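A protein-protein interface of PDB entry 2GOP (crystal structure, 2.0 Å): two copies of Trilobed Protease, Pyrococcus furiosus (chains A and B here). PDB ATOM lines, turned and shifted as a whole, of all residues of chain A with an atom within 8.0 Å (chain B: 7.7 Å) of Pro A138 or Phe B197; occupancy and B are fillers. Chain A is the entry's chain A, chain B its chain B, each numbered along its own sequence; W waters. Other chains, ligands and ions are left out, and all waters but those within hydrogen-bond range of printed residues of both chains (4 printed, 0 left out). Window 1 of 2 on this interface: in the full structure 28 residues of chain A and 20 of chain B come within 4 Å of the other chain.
The backbone NH (N) of Ile A304 lies within hydrogen-bond range of the backbone carbonyl oxygen (O) of Val A285 (2.9 Å). O of Glu A318 sits at hydrogen-bond distance from N of Trp A303 (2.8 Å). OE1 of Glu A318 is in salt-bridge range of NH1 of Arg A324 (3.0 Å). The indole nitrogen (NE1) of Trp A303 sits close to the side-chain sulfur (SD) of Met A305 (3.7 Å). OG1 of Thr A278 lies within hydrogen-bond range of N of Gln A267 (3.0 Å). The backbone carbonyl oxygen (O) of Met A305 sits at hydrogen-bond distance from the indole nitrogen (NE1) of Trp A140 (2.9 Å).
Hydrophobic or aromatic side chains of chain A that line the printed part of chain B: Pro A138, Trp A140, Phe A280, Val A285, Trp A303 and Met A305. Of the 16 printed residues of chain B, 7 touch a printed residue of chain A. Printed residues of chain B that touch a printed residue of chain A: Pro B194, Gln B195, Tyr B196, Phe B197, Tyr B239, Met B240 and Ser B241. Hydrophobic or aromatic side chains of chain B that line the printed part of chain A: Tyr B196, Phe B197, Tyr B239 and Met B240. Among the printed residues, no Asp or Glu carboxylate lies within 4 Å of a Lys or Arg side-chain nitrogen of the other chain.
The side-chain carboxylate (OE2) of Glu A318 lies within hydrogen-bond range of the side-chain hydroxyl (OH) of Tyr B239 (3.1 Å). N of Ala A139 is in hydrogen-bond range of O of Tyr B196, 2.9 Å away. The side-chain hydroxyl (OH) of Tyr B196 is in hydrogen-bond range of the backbone NH (N) of Gly A306. The backbone carbonyl oxygen of Ala A139 lies close to the backbone carbonyl oxygen of Gln B195.
No position is printed for both chains. Of the 16 pairs that touch across the chains among the printed residues, none has its exchanged pair printed and touching as well.
Pro A138 touches Tyr B196. CG of Pro A138 touches CD1 of Phe B197 (3.6 Å). CZ3 of Trp A140 touches O of Pro B194, 3.5 Å away. CZ3 of Trp A140 touches C of Gln B195 (3.4 Å). Trp A140 touches Tyr B196 (CZ3 to N, 3.4 Å). Gln A267 touches Tyr B196. Ser B241 touches Phe A280 (O to CD2, 3.9 Å). Val A285 touches Met B240. Trp A303 touches Tyr B239. Tyr B196 touches Met A305.
Water W3 lies within hydrogen-bond range of the side-chain hydroxyl of Tyr B196 (2.6 Å), the side-chain hydroxyl of Thr A278 (3.1 Å) and the backbone NH of Gln A267 (3.3 Å). Water W2 bridges OE2 of Glu A318 (2.6 Å) and OH of Tyr B239 (2.7 Å). Water W4 lies within hydrogen-bond range of OE1 of Gln A267 and OH of Tyr B196. Water W1 bridges O of Pro B194 (2.8 Å) and NH2 of Arg A324 (3.0 Å).
Pro A138 touches two residues of chain B. Of the printed residues of chain B, Gly A306 touches Tyr B196 (3.5 Å). Printed residues of chain A within 4 Å of Gln B195: Ala A139 and Trp A140. Phe B197 touches one residue of chain A. Lys B234 touches none of the printed residues of chain A.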
ATOM      1  N   VAL A 137      -1.313  -9.304  -8.399  1.00  0.00           N
ATOM      2  CA  VAL A 137      -2.343  -9.629  -9.380  1.00  0.00           C
ATOM      3  C   VAL A 137      -2.275  -8.661 -10.567  1.00  0.00           C
ATOM      4  O   VAL A 137      -2.972  -7.648 -10.588  1.00  0.00           O
ATOM      5  CB  VAL A 137      -3.760  -9.589  -8.744  1.00  0.00           C
ATOM      6  CG1 VAL A 137      -4.820 -10.042  -9.745  1.00  0.00           C
ATOM      7  CG2 VAL A 137      -3.809 -10.453  -7.503  1.00  0.00           C
ATOM      8  N   PRO A 138      -1.404  -8.953 -11.549  1.00  0.00           N
ATOM      9  CA  PRO A 138      -1.407  -8.213 -12.811  1.00  0.00           C
ATOM     10  C   PRO A 138      -2.804  -8.076 -13.438  1.00  0.00           C
ATOM     11  O   PRO A 138      -3.613  -9.010 -13.383  1.00  0.00           O
ATOM     12  CB  PRO A 138      -0.486  -9.052 -13.708  1.00  0.00           C
ATOM     13  CG  PRO A 138       0.462  -9.688 -12.764  1.00  0.00           C
ATOM     14  CD  PRO A 138      -0.330  -9.963 -11.508  1.00  0.00           C
ATOM     15  N   ALA A 139      -3.073  -6.905 -14.015  1.00  0.00           N
ATOM     16  CA  ALA A 139      -4.367  -6.597 -14.623  1.00  0.00           C
ATOM     17  C   ALA A 139      -4.263  -5.272 -15.381  1.00  0.00           C
ATOM     18  O   ALA A 139      -3.445  -4.430 -15.033  1.00  0.00           O
ATOM     19  CB  ALA A 139      -5.456  -6.516 -13.545  1.00  0.00           C
ATOM     20  N   TRP A 140      -5.094  -5.087 -16.407  1.00  0.00           N
ATOM     21  CA  TRP A 140      -5.066  -3.852 -17.211  1.00  0.00           C
ATOM     22  C   TRP A 140      -5.729  -2.652 -16.525  1.00  0.00           C
ATOM     23  O   TRP A 140      -5.996  -2.672 -15.323  1.00  0.00           O
ATOM     24  CB  TRP A 140      -5.724  -4.081 -18.573  1.00  0.00           C
ATOM     25  CG  TRP A 140      -4.893  -4.887 -19.497  1.00  0.00           C
ATOM     26  CD1 TRP A 140      -5.200  -6.103 -20.029  1.00  0.00           C
ATOM     27  CD2 TRP A 140      -3.599  -4.546 -19.997  1.00  0.00           C
ATOM     28  NE1 TRP A 140      -4.182  -6.538 -20.843  1.00  0.00           N
ATOM     29  CE2 TRP A 140      -3.187  -5.600 -20.845  1.00  0.00           C
ATOM     30  CE3 TRP A 140      -2.751  -3.446 -19.823  1.00  0.00           C
ATOM     31  CZ2 TRP A 140      -1.957  -5.589 -21.509  1.00  0.00           C
ATOM     32  CZ3 TRP A 140      -1.529  -3.437 -20.483  1.00  0.00           C
ATOM     33  CH2 TRP A 140      -1.146  -4.502 -21.316  1.00  0.00           C
ATOM     34  N   TYR A 232     -11.368 -16.545  -6.195  1.00  0.00           N
ATOM     35  CA  TYR A 232      -9.922 -16.414  -6.312  1.00  0.00           C
ATOM     36  C   TYR A 232      -9.330 -16.119  -4.932  1.00  0.00           C
ATOM     37  O   TYR A 232      -9.808 -15.233  -4.226  1.00  0.00           O
ATOM     38  CB  TYR A 232      -9.631 -15.251  -7.254  1.00  0.00           C
ATOM     39  CG  TYR A 232      -8.183 -15.016  -7.634  1.00  0.00           C
ATOM     40  CD1 TYR A 232      -7.605 -15.694  -8.702  1.00  0.00           C
ATOM     41  CD2 TYR A 232      -7.411 -14.055  -6.984  1.00  0.00           C
ATOM     42  CE1 TYR A 232      -6.276 -15.451  -9.087  1.00  0.00           C
ATOM     43  CE2 TYR A 232      -6.098 -13.800  -7.369  1.00  0.00           C
ATOM     44  CZ  TYR A 232      -5.535 -14.502  -8.423  1.00  0.00           C
ATOM     45  OH  TYR A 232      -4.212 -14.264  -8.807  1.00  0.00           O
ATOM     46  N   VAL A 265      -1.582 -18.188 -10.413  1.00  0.00           N
ATOM     47  CA  VAL A 265      -2.680 -17.944 -11.347  1.00  0.00           C
ATOM     48  C   VAL A 265      -2.769 -16.451 -11.625  1.00  0.00           C
ATOM     49  O   VAL A 265      -2.668 -15.661 -10.717  1.00  0.00           O
ATOM     50  CB  VAL A 265      -4.051 -18.411 -10.756  1.00  0.00           C
ATOM     51  CG1 VAL A 265      -5.220 -18.058 -11.703  1.00  0.00           C
ATOM     52  CG2 VAL A 265      -4.039 -19.892 -10.470  1.00  0.00           C
ATOM     53  N   GLY A 266      -2.959 -16.072 -12.881  1.00  0.00           N
ATOM     54  CA  GLY A 266      -3.209 -14.679 -13.244  1.00  0.00           C
ATOM     55  C   GLY A 266      -4.704 -14.413 -13.288  1.00  0.00           C
ATOM     56  O   GLY A 266      -5.377 -14.501 -12.276  1.00  0.00           O
ATOM     57  N   GLN A 267      -5.227 -14.129 -14.473  1.00  0.00           N
ATOM     58  CA  GLN A 267      -6.636 -13.839 -14.658  1.00  0.00           C
ATOM     59  C   GLN A 267      -7.399 -15.152 -14.889  1.00  0.00           C
ATOM     60  O   GLN A 267      -6.841 -16.107 -15.403  1.00  0.00           O
ATOM     61  CB  GLN A 267      -6.798 -12.892 -15.856  1.00  0.00           C
ATOM     62  CG  GLN A 267      -8.225 -12.456 -16.149  1.00  0.00           C
ATOM     63  CD  GLN A 267      -8.373 -11.735 -17.494  1.00  0.00           C
ATOM     64  OE1 GLN A 267      -7.399 -11.510 -18.211  1.00  0.00           O
ATOM     65  NE2 GLN A 267      -9.607 -11.387 -17.837  1.00  0.00           N
ATOM     66  N   THR A 278      -5.022 -18.191 -16.673  1.00  0.00           N
ATOM     67  CA  THR A 278      -3.601 -18.120 -16.973  1.00  0.00           C
ATOM     68  C   THR A 278      -2.799 -18.612 -15.781  1.00  0.00           C
ATOM     69  O   THR A 278      -3.174 -18.402 -14.623  1.00  0.00           O
ATOM     70  CB  THR A 278      -3.141 -16.694 -17.348  1.00  0.00           C
ATOM     71  OG1 THR A 278      -3.440 -15.789 -16.282  1.00  0.00           O
ATOM     72  CG2 THR A 278      -3.829 -16.217 -18.633  1.00  0.00           C
ATOM     73  N   PHE A 280       1.354 -18.850 -14.326  1.00  0.00           N
ATOM     74  CA  PHE A 280       2.750 -18.423 -14.407  1.00  0.00           C
ATOM     75  C   PHE A 280       3.636 -19.664 -14.224  1.00  0.00           C
ATOM     76  O   PHE A 280       3.654 -20.259 -13.143  1.00  0.00           O
ATOM     77  CB  PHE A 280       3.074 -17.399 -13.322  1.00  0.00           C
ATOM     78  CG  PHE A 280       2.496 -16.029 -13.573  1.00  0.00           C
ATOM     79  CD1 PHE A 280       1.124 -15.823 -13.556  1.00  0.00           C
ATOM     80  CD2 PHE A 280       3.327 -14.946 -13.801  1.00  0.00           C
ATOM     81  CE1 PHE A 280       0.593 -14.564 -13.777  1.00  0.00           C
ATOM     82  CE2 PHE A 280       2.806 -13.682 -14.023  1.00  0.00           C
ATOM     83  CZ  PHE A 280       1.434 -13.489 -14.010  1.00  0.00           C
ATOM     84  N   VAL A 285       3.733 -17.192 -19.266  1.00  0.00           N
ATOM     85  CA  VAL A 285       2.376 -17.057 -18.769  1.00  0.00           C
ATOM     86  C   VAL A 285       1.472 -17.683 -19.826  1.00  0.00           C
ATOM     87  O   VAL A 285       1.362 -17.169 -20.937  1.00  0.00           O
ATOM     88  CB  VAL A 285       2.023 -15.587 -18.501  1.00  0.00           C
ATOM     89  CG1 VAL A 285       0.575 -15.451 -17.968  1.00  0.00           C
ATOM     90  CG2 VAL A 285       3.042 -14.973 -17.523  1.00  0.00           C
ATOM     91  N   TRP A 303       4.142 -14.734 -23.032  1.00  0.00           N
ATOM     92  CA  TRP A 303       3.230 -14.396 -21.955  1.00  0.00           C
ATOM     93  C   TRP A 303       1.901 -13.855 -22.465  1.00  0.00           C
ATOM     94  O   TRP A 303       1.844 -12.932 -23.291  1.00  0.00           O
ATOM     95  CB  TRP A 303       3.863 -13.509 -20.862  1.00  0.00           C
ATOM     96  CG  TRP A 303       4.670 -12.340 -21.281  1.00  0.00           C
ATOM     97  CD1 TRP A 303       4.326 -11.017 -21.157  1.00  0.00           C
ATOM     98  CD2 TRP A 303       5.992 -12.361 -21.842  1.00  0.00           C
ATOM     99  NE1 TRP A 303       5.345 -10.218 -21.629  1.00  0.00           N
ATOM    100  CE2 TRP A 303       6.375 -11.019 -22.059  1.00  0.00           C
ATOM    101  CE3 TRP A 303       6.880 -13.381 -22.201  1.00  0.00           C
ATOM    102  CZ2 TRP A 303       7.614 -10.676 -22.614  1.00  0.00           C
ATOM    103  CZ3 TRP A 303       8.109 -13.036 -22.743  1.00  0.00           C
ATOM    104  CH2 TRP A 303       8.459 -11.693 -22.950  1.00  0.00           C
ATOM    105  N   ILE A 304       0.837 -14.480 -21.966  1.00  0.00           N
ATOM    106  CA  ILE A 304      -0.524 -14.041 -22.229  1.00  0.00           C
ATOM    107  C   ILE A 304      -0.834 -12.864 -21.309  1.00  0.00           C
ATOM    108  O   ILE A 304      -0.758 -12.988 -20.091  1.00  0.00           O
ATOM    109  CB  ILE A 304      -1.538 -15.183 -21.997  1.00  0.00           C
ATOM    110  CG1 ILE A 304      -1.222 -16.392 -22.895  1.00  0.00           C
ATOM    111  CG2 ILE A 304      -2.957 -14.689 -22.218  1.00  0.00           C
ATOM    112  CD1 ILE A 304      -1.283 -16.139 -24.411  1.00  0.00           C
ATOM    113  N   MET A 305      -1.160 -11.719 -21.900  1.00  0.00           N
ATOM    114  CA  MET A 305      -1.403 -10.497 -21.150  1.00  0.00           C
ATOM    115  C   MET A 305      -2.860 -10.082 -21.267  1.00  0.00           C
ATOM    116  O   MET A 305      -3.198  -9.096 -21.920  1.00  0.00           O
ATOM    117  CB  MET A 305      -0.479  -9.385 -21.650  1.00  0.00           C
ATOM    118  CG  MET A 305       0.995  -9.671 -21.357  1.00  0.00           C
ATOM    119  SD  MET A 305       2.090  -8.402 -22.000  1.00  0.00           S
ATOM    120  CE  MET A 305       1.581  -6.985 -21.040  1.00  0.00           C
ATOM    121  N   GLY A 306      -3.723 -10.845 -20.610  1.00  0.00           N
ATOM    122  CA  GLY A 306      -5.156 -10.616 -20.663  1.00  0.00           C
ATOM    123  C   GLY A 306      -5.837 -11.417 -21.764  1.00  0.00           C
ATOM    124  O   GLY A 306      -5.277 -11.638 -22.845  1.00  0.00           O
ATOM    125  N   GLU A 318       2.411 -11.770 -25.888  1.00  0.00           N
ATOM    126  CA  GLU A 318       3.705 -11.130 -26.040  1.00  0.00           C
ATOM    127  C   GLU A 318       4.827 -12.168 -26.006  1.00  0.00           C
ATOM    128  O   GLU A 318       4.710 -13.197 -25.345  1.00  0.00           O
ATOM    129  CB  GLU A 318       3.903 -10.116 -24.918  1.00  0.00           C
ATOM    130  CG  GLU A 318       5.124  -9.240 -25.073  1.00  0.00           C
ATOM    131  CD  GLU A 318       4.936  -7.896 -24.435  1.00  0.00           C
ATOM    132  OE1 GLU A 318       4.094  -7.124 -24.938  1.00  0.00           O
ATOM    133  OE2 GLU A 318       5.631  -7.608 -23.438  1.00  0.00           O
ATOM    134  N   ARG A 324       3.088  -7.483 -27.578  1.00  0.00           N
ATOM    135  CA  ARG A 324       1.776  -8.113 -27.628  1.00  0.00           C
ATOM    136  C   ARG A 324       0.954  -7.704 -28.855  1.00  0.00           C
ATOM    137  O   ARG A 324       0.928  -6.534 -29.245  1.00  0.00           O
ATOM    138  CB  ARG A 324       0.989  -7.834 -26.346  1.00  0.00           C
ATOM    139  CG  ARG A 324       0.810  -6.362 -26.019  1.00  0.00           C
ATOM    140  CD  ARG A 324       0.667  -6.130 -24.528  1.00  0.00           C
ATOM    141  NE  ARG A 324       0.685  -4.704 -24.199  1.00  0.00           N
ATOM    142  CZ  ARG A 324       1.776  -3.980 -23.958  1.00  0.00           C
ATOM    143  NH1 ARG A 324       2.989  -4.512 -24.001  1.00  0.00           N
ATOM    144  NH2 ARG A 324       1.647  -2.697 -23.662  1.00  0.00           N
ATOM    145  N   HIS B 189       5.762   3.163 -10.221  1.00  0.00           N
ATOM    146  CA  HIS B 189       6.070   3.748 -11.510  1.00  0.00           C
ATOM    147  C   HIS B 189       4.778   4.244 -12.163  1.00  0.00           C
ATOM    148  O   HIS B 189       3.824   3.485 -12.333  1.00  0.00           O
ATOM    149  CB  HIS B 189       6.775   2.741 -12.414  1.00  0.00           C
ATOM    150  CG  HIS B 189       7.091   3.281 -13.772  1.00  0.00           C
ATOM    151  ND1 HIS B 189       8.038   4.260 -13.979  1.00  0.00           N
ATOM    152  CD2 HIS B 189       6.567   2.997 -14.987  1.00  0.00           C
ATOM    153  CE1 HIS B 189       8.091   4.552 -15.267  1.00  0.00           C
ATOM    154  NE2 HIS B 189       7.206   3.800 -15.900  1.00  0.00           N
ATOM    155  N   GLU B 191       2.818   5.687 -15.396  1.00  0.00           N
ATOM    156  CA  GLU B 191       2.899   5.612 -16.859  1.00  0.00           C
ATOM    157  C   GLU B 191       1.616   6.096 -17.515  1.00  0.00           C
ATOM    158  O   GLU B 191       0.530   5.913 -16.969  1.00  0.00           O
ATOM    159  CB  GLU B 191       3.160   4.172 -17.307  1.00  0.00           C
ATOM    160  CG  GLU B 191       3.873   4.054 -18.649  1.00  0.00           C
ATOM    161  CD  GLU B 191       5.339   3.713 -18.487  1.00  0.00           C
ATOM    162  OE1 GLU B 191       6.196   4.620 -18.630  1.00  0.00           O
ATOM    163  OE2 GLU B 191       5.632   2.533 -18.188  1.00  0.00           O
ATOM    164  N   PRO B 194      -1.069   2.238 -20.788  1.00  0.00           N
ATOM    165  CA  PRO B 194      -1.636   1.260 -19.854  1.00  0.00           C
ATOM    166  C   PRO B 194      -0.680   0.099 -19.578  1.00  0.00           C
ATOM    167  O   PRO B 194       0.071  -0.329 -20.461  1.00  0.00           O
ATOM    168  CB  PRO B 194      -2.915   0.782 -20.558  1.00  0.00           C
ATOM    169  CG  PRO B 194      -3.278   1.889 -21.477  1.00  0.00           C
ATOM    170  CD  PRO B 194      -1.951   2.458 -21.951  1.00  0.00           C
ATOM    171  N   GLN B 195      -0.692  -0.379 -18.343  1.00  0.00           N
ATOM    172  CA  GLN B 195       0.244  -1.410 -17.917  1.00  0.00           C
ATOM    173  C   GLN B 195      -0.514  -2.593 -17.333  1.00  0.00           C
ATOM    174  O   GLN B 195      -1.583  -2.425 -16.744  1.00  0.00           O
ATOM    175  CB  GLN B 195       1.220  -0.834 -16.890  1.00  0.00           C
ATOM    176  CG  GLN B 195       2.664  -1.278 -17.071  1.00  0.00           C
ATOM    177  CD  GLN B 195       3.330  -0.732 -18.333  1.00  0.00           C
ATOM    178  OE1 GLN B 195       4.318  -1.291 -18.805  1.00  0.00           O
ATOM    179  NE2 GLN B 195       2.799   0.362 -18.876  1.00  0.00           N
ATOM    180  N   TYR B 196       0.056  -3.779 -17.515  1.00  0.00           N
ATOM    181  CA  TYR B 196      -0.503  -5.024 -17.006  1.00  0.00           C
ATOM    182  C   TYR B 196       0.164  -5.431 -15.691  1.00  0.00           C
ATOM    183  O   TYR B 196      -0.488  -5.973 -14.809  1.00  0.00           O
ATOM    184  CB  TYR B 196      -0.316  -6.136 -18.039  1.00  0.00           C
ATOM    185  CG  TYR B 196      -1.190  -7.343 -17.805  1.00  0.00           C
ATOM    186  CD1 TYR B 196      -2.574  -7.213 -17.740  1.00  0.00           C
ATOM    187  CD2 TYR B 196      -0.643  -8.616 -17.659  1.00  0.00           C
ATOM    188  CE1 TYR B 196      -3.395  -8.316 -17.524  1.00  0.00           C
ATOM    189  CE2 TYR B 196      -1.464  -9.731 -17.442  1.00  0.00           C
ATOM    190  CZ  TYR B 196      -2.832  -9.567 -17.380  1.00  0.00           C
ATOM    191  OH  TYR B 196      -3.650 -10.646 -17.162  1.00  0.00           O
ATOM    192  N   PHE B 197       1.463  -5.175 -15.588  1.00  0.00           N
ATOM    193  CA  PHE B 197       2.257  -5.500 -14.410  1.00  0.00           C
ATOM    194  C   PHE B 197       2.543  -4.227 -13.606  1.00  0.00           C
ATOM    195  O   PHE B 197       2.485  -3.117 -14.146  1.00  0.00           O
ATOM    196  CB  PHE B 197       3.572  -6.159 -14.838  1.00  0.00           C
ATOM    197  CG  PHE B 197       3.391  -7.466 -15.585  1.00  0.00           C
ATOM    198  CD1 PHE B 197       3.226  -8.667 -14.892  1.00  0.00           C
ATOM    199  CD2 PHE B 197       3.409  -7.500 -16.975  1.00  0.00           C
ATOM    200  CE1 PHE B 197       3.073  -9.877 -15.574  1.00  0.00           C
ATOM    201  CE2 PHE B 197       3.250  -8.711 -17.660  1.00  0.00           C
ATOM    202  CZ  PHE B 197       3.085  -9.898 -16.954  1.00  0.00           C
ATOM    203  N   LYS B 198       2.854  -4.388 -12.321  1.00  0.00           N
ATOM    204  CA  LYS B 198       3.142  -3.237 -11.457  1.00  0.00           C
ATOM    205  C   LYS B 198       4.653  -3.026 -11.338  1.00  0.00           C
ATOM    206  O   LYS B 198       5.406  -3.961 -11.062  1.00  0.00           O
ATOM    207  CB  LYS B 198       2.465  -3.372 -10.079  1.00  0.00           C
ATOM    208  CG  LYS B 198       2.997  -4.475  -9.154  1.00  0.00           C
ATOM    209  CD  LYS B 198       2.623  -4.202  -7.677  1.00  0.00           C
ATOM    210  CE  LYS B 198       3.241  -5.227  -6.725  1.00  0.00           C
ATOM    211  NZ  LYS B 198       3.086  -4.857  -5.290  1.00  0.00           N
ATOM    212  N   PHE B 199       5.083  -1.791 -11.575  1.00  0.00           N
ATOM    213  CA  PHE B 199       6.502  -1.453 -11.606  1.00  0.00           C
ATOM    214  C   PHE B 199       6.837  -0.386 -10.576  1.00  0.00           C
ATOM    215  O   PHE B 199       5.959   0.307 -10.071  1.00  0.00           O
ATOM    216  CB  PHE B 199       6.896  -0.966 -13.002  1.00  0.00           C
ATOM    217  CG  PHE B 199       6.798  -2.021 -14.061  1.00  0.00           C
ATOM    218  CD1 PHE B 199       7.803  -2.970 -14.209  1.00  0.00           C
ATOM    219  CD2 PHE B 199       5.704  -2.068 -14.918  1.00  0.00           C
ATOM    220  CE1 PHE B 199       7.710  -3.958 -15.196  1.00  0.00           C
ATOM    221  CE2 PHE B 199       5.609  -3.048 -15.908  1.00  0.00           C
ATOM    222  CZ  PHE B 199       6.614  -3.994 -16.043  1.00  0.00           C
ATOM    223  N   TRP B 200       8.128  -0.237 -10.308  1.00  0.00           N
ATOM    224  CA  TRP B 200       8.617   0.659  -9.265  1.00  0.00           C
ATOM    225  C   TRP B 200       9.733   1.548  -9.777  1.00  0.00           C
ATOM    226  O   TRP B 200      10.538   1.122 -10.606  1.00  0.00           O
ATOM    227  CB  TRP B 200       9.131  -0.172  -8.088  1.00  0.00           C
ATOM    228  CG  TRP B 200       8.032  -0.899  -7.406  1.00  0.00           C
ATOM    229  CD1 TRP B 200       7.596  -2.175  -7.666  1.00  0.00           C
ATOM    230  CD2 TRP B 200       7.178  -0.385  -6.384  1.00  0.00           C
ATOM    231  NE1 TRP B 200       6.542  -2.489  -6.843  1.00  0.00           N
ATOM    232  CE2 TRP B 200       6.259  -1.407  -6.052  1.00  0.00           C
ATOM    233  CE3 TRP B 200       7.112   0.831  -5.701  1.00  0.00           C
ATOM    234  CZ2 TRP B 200       5.290  -1.247  -5.068  1.00  0.00           C
ATOM    235  CZ3 TRP B 200       6.142   0.992  -4.720  1.00  0.00           C
ATOM    236  CH2 TRP B 200       5.242  -0.043  -4.414  1.00  0.00           C
ATOM    237  N   LYS B 216      11.296   2.110 -13.538  1.00  0.00           N
ATOM    238  CA  LYS B 216      10.414   1.049 -14.022  1.00  0.00           C
ATOM    239  C   LYS B 216      11.035  -0.347 -13.854  1.00  0.00           C
ATOM    240  O   LYS B 216      11.289  -1.051 -14.830  1.00  0.00           O
ATOM    241  CB  LYS B 216      10.014   1.294 -15.489  1.00  0.00           C
ATOM    242  CG  LYS B 216       8.911   0.357 -15.996  1.00  0.00           C
ATOM    243  CD  LYS B 216       8.387   0.763 -17.358  1.00  0.00           C
ATOM    244  CE  LYS B 216       7.272  -0.169 -17.818  1.00  0.00           C
ATOM    245  NZ  LYS B 216       6.763   0.176 -19.171  1.00  0.00           N
ATOM    246  N   SER B 218      10.920  -4.166 -11.419  1.00  0.00           N
ATOM    247  CA  SER B 218       9.948  -5.082 -10.850  1.00  0.00           C
ATOM    248  C   SER B 218      10.400  -5.599  -9.494  1.00  0.00           C
ATOM    249  O   SER B 218       9.939  -6.638  -9.029  1.00  0.00           O
ATOM    250  CB  SER B 218       9.728  -6.252 -11.813  1.00  0.00           C
ATOM    251  OG  SER B 218       9.256  -5.775 -13.057  1.00  0.00           O
ATOM    252  N   LYS B 234      11.142  -9.253  -8.789  1.00  0.00           N
ATOM    253  CA  LYS B 234      11.504  -9.929 -10.019  1.00  0.00           C
ATOM    254  C   LYS B 234      12.558  -9.155 -10.792  1.00  0.00           C
ATOM    255  O   LYS B 234      12.660  -7.930 -10.657  1.00  0.00           O
ATOM    256  CB  LYS B 234      10.253 -10.154 -10.869  1.00  0.00           C
ATOM    257  CG  LYS B 234       9.409 -11.293 -10.329  1.00  0.00           C
ATOM    258  CD  LYS B 234       7.937 -11.115 -10.566  1.00  0.00           C
ATOM    259  CE  LYS B 234       7.139 -12.090  -9.698  1.00  0.00           C
ATOM    260  NZ  LYS B 234       5.845 -12.469 -10.321  1.00  0.00           N
ATOM    261  N   LYS B 238      12.321  -9.654 -16.772  1.00  0.00           N
ATOM    262  CA  LYS B 238      11.617 -10.891 -16.431  1.00  0.00           C
ATOM    263  C   LYS B 238      10.517 -10.608 -15.402  1.00  0.00           C
ATOM    264  O   LYS B 238      10.294 -11.383 -14.471  1.00  0.00           O
ATOM    265  CB  LYS B 238      12.593 -11.961 -15.928  1.00  0.00           C
ATOM    266  CG  LYS B 238      13.764 -12.242 -16.876  1.00  0.00           C
ATOM    267  CD  LYS B 238      13.301 -12.794 -18.220  1.00  0.00           C
ATOM    268  CE  LYS B 238      14.463 -12.968 -19.187  1.00  0.00           C
ATOM    269  NZ  LYS B 238      15.067 -11.667 -19.595  1.00  0.00           N
ATOM    270  N   TYR B 239       9.833  -9.482 -15.599  1.00  0.00           N
ATOM    271  CA  TYR B 239       8.663  -9.089 -14.802  1.00  0.00           C
ATOM    272  C   TYR B 239       7.510 -10.100 -14.863  1.00  0.00           C
ATOM    273  O   TYR B 239       6.637 -10.086 -14.000  1.00  0.00           O
ATOM    274  CB  TYR B 239       8.161  -7.693 -15.243  1.00  0.00           C
ATOM    275  CG  TYR B 239       7.936  -7.559 -16.734  1.00  0.00           C
ATOM    276  CD1 TYR B 239       6.752  -7.990 -17.321  1.00  0.00           C
ATOM    277  CD2 TYR B 239       8.923  -7.025 -17.557  1.00  0.00           C
ATOM    278  CE1 TYR B 239       6.549  -7.887 -18.686  1.00  0.00           C
ATOM    279  CE2 TYR B 239       8.734  -6.917 -18.926  1.00  0.00           C
ATOM    280  CZ  TYR B 239       7.545  -7.348 -19.488  1.00  0.00           C
ATOM    281  OH  TYR B 239       7.353  -7.238 -20.851  1.00  0.00           O
ATOM    282  N   MET B 240       7.509 -10.969 -15.874  1.00  0.00           N
ATOM    283  CA  MET B 240       6.490 -12.013 -16.009  1.00  0.00           C
ATOM    284  C   MET B 240       6.862 -13.317 -15.286  1.00  0.00           C
ATOM    285  O   MET B 240       6.172 -14.332 -15.440  1.00  0.00           O
ATOM    286  CB  MET B 240       6.209 -12.292 -17.495  1.00  0.00           C
ATOM    287  CG  MET B 240       7.275 -13.126 -18.236  1.00  0.00           C
ATOM    288  SD  MET B 240       8.936 -12.396 -18.296  1.00  0.00           S
ATOM    289  CE  MET B 240       8.655 -10.898 -19.251  1.00  0.00           C
ATOM    290  N   SER B 241       7.946 -13.293 -14.511  1.00  0.00           N
ATOM    291  CA  SER B 241       8.423 -14.487 -13.817  1.00  0.00           C
ATOM    292  C   SER B 241       7.511 -14.910 -12.676  1.00  0.00           C
ATOM    293  O   SER B 241       6.750 -14.115 -12.137  1.00  0.00           O
ATOM    294  CB  SER B 241       9.835 -14.273 -13.274  1.00  0.00           C
ATOM    295  OG  SER B 241      10.772 -14.214 -14.333  1.00  0.00           O
HETATM  296  O   HOH W   1      -0.705  -0.954 -23.108  1.00  0.00           O
HETATM  297  O   HOH W   2       5.820  -5.397 -22.089  1.00  0.00           O
HETATM  298  O   HOH W   3      -2.679 -12.783 -16.120  1.00  0.00           O
HETATM  299  O   HOH W   4      -6.219  -9.799 -16.503  1.00  0.00           O
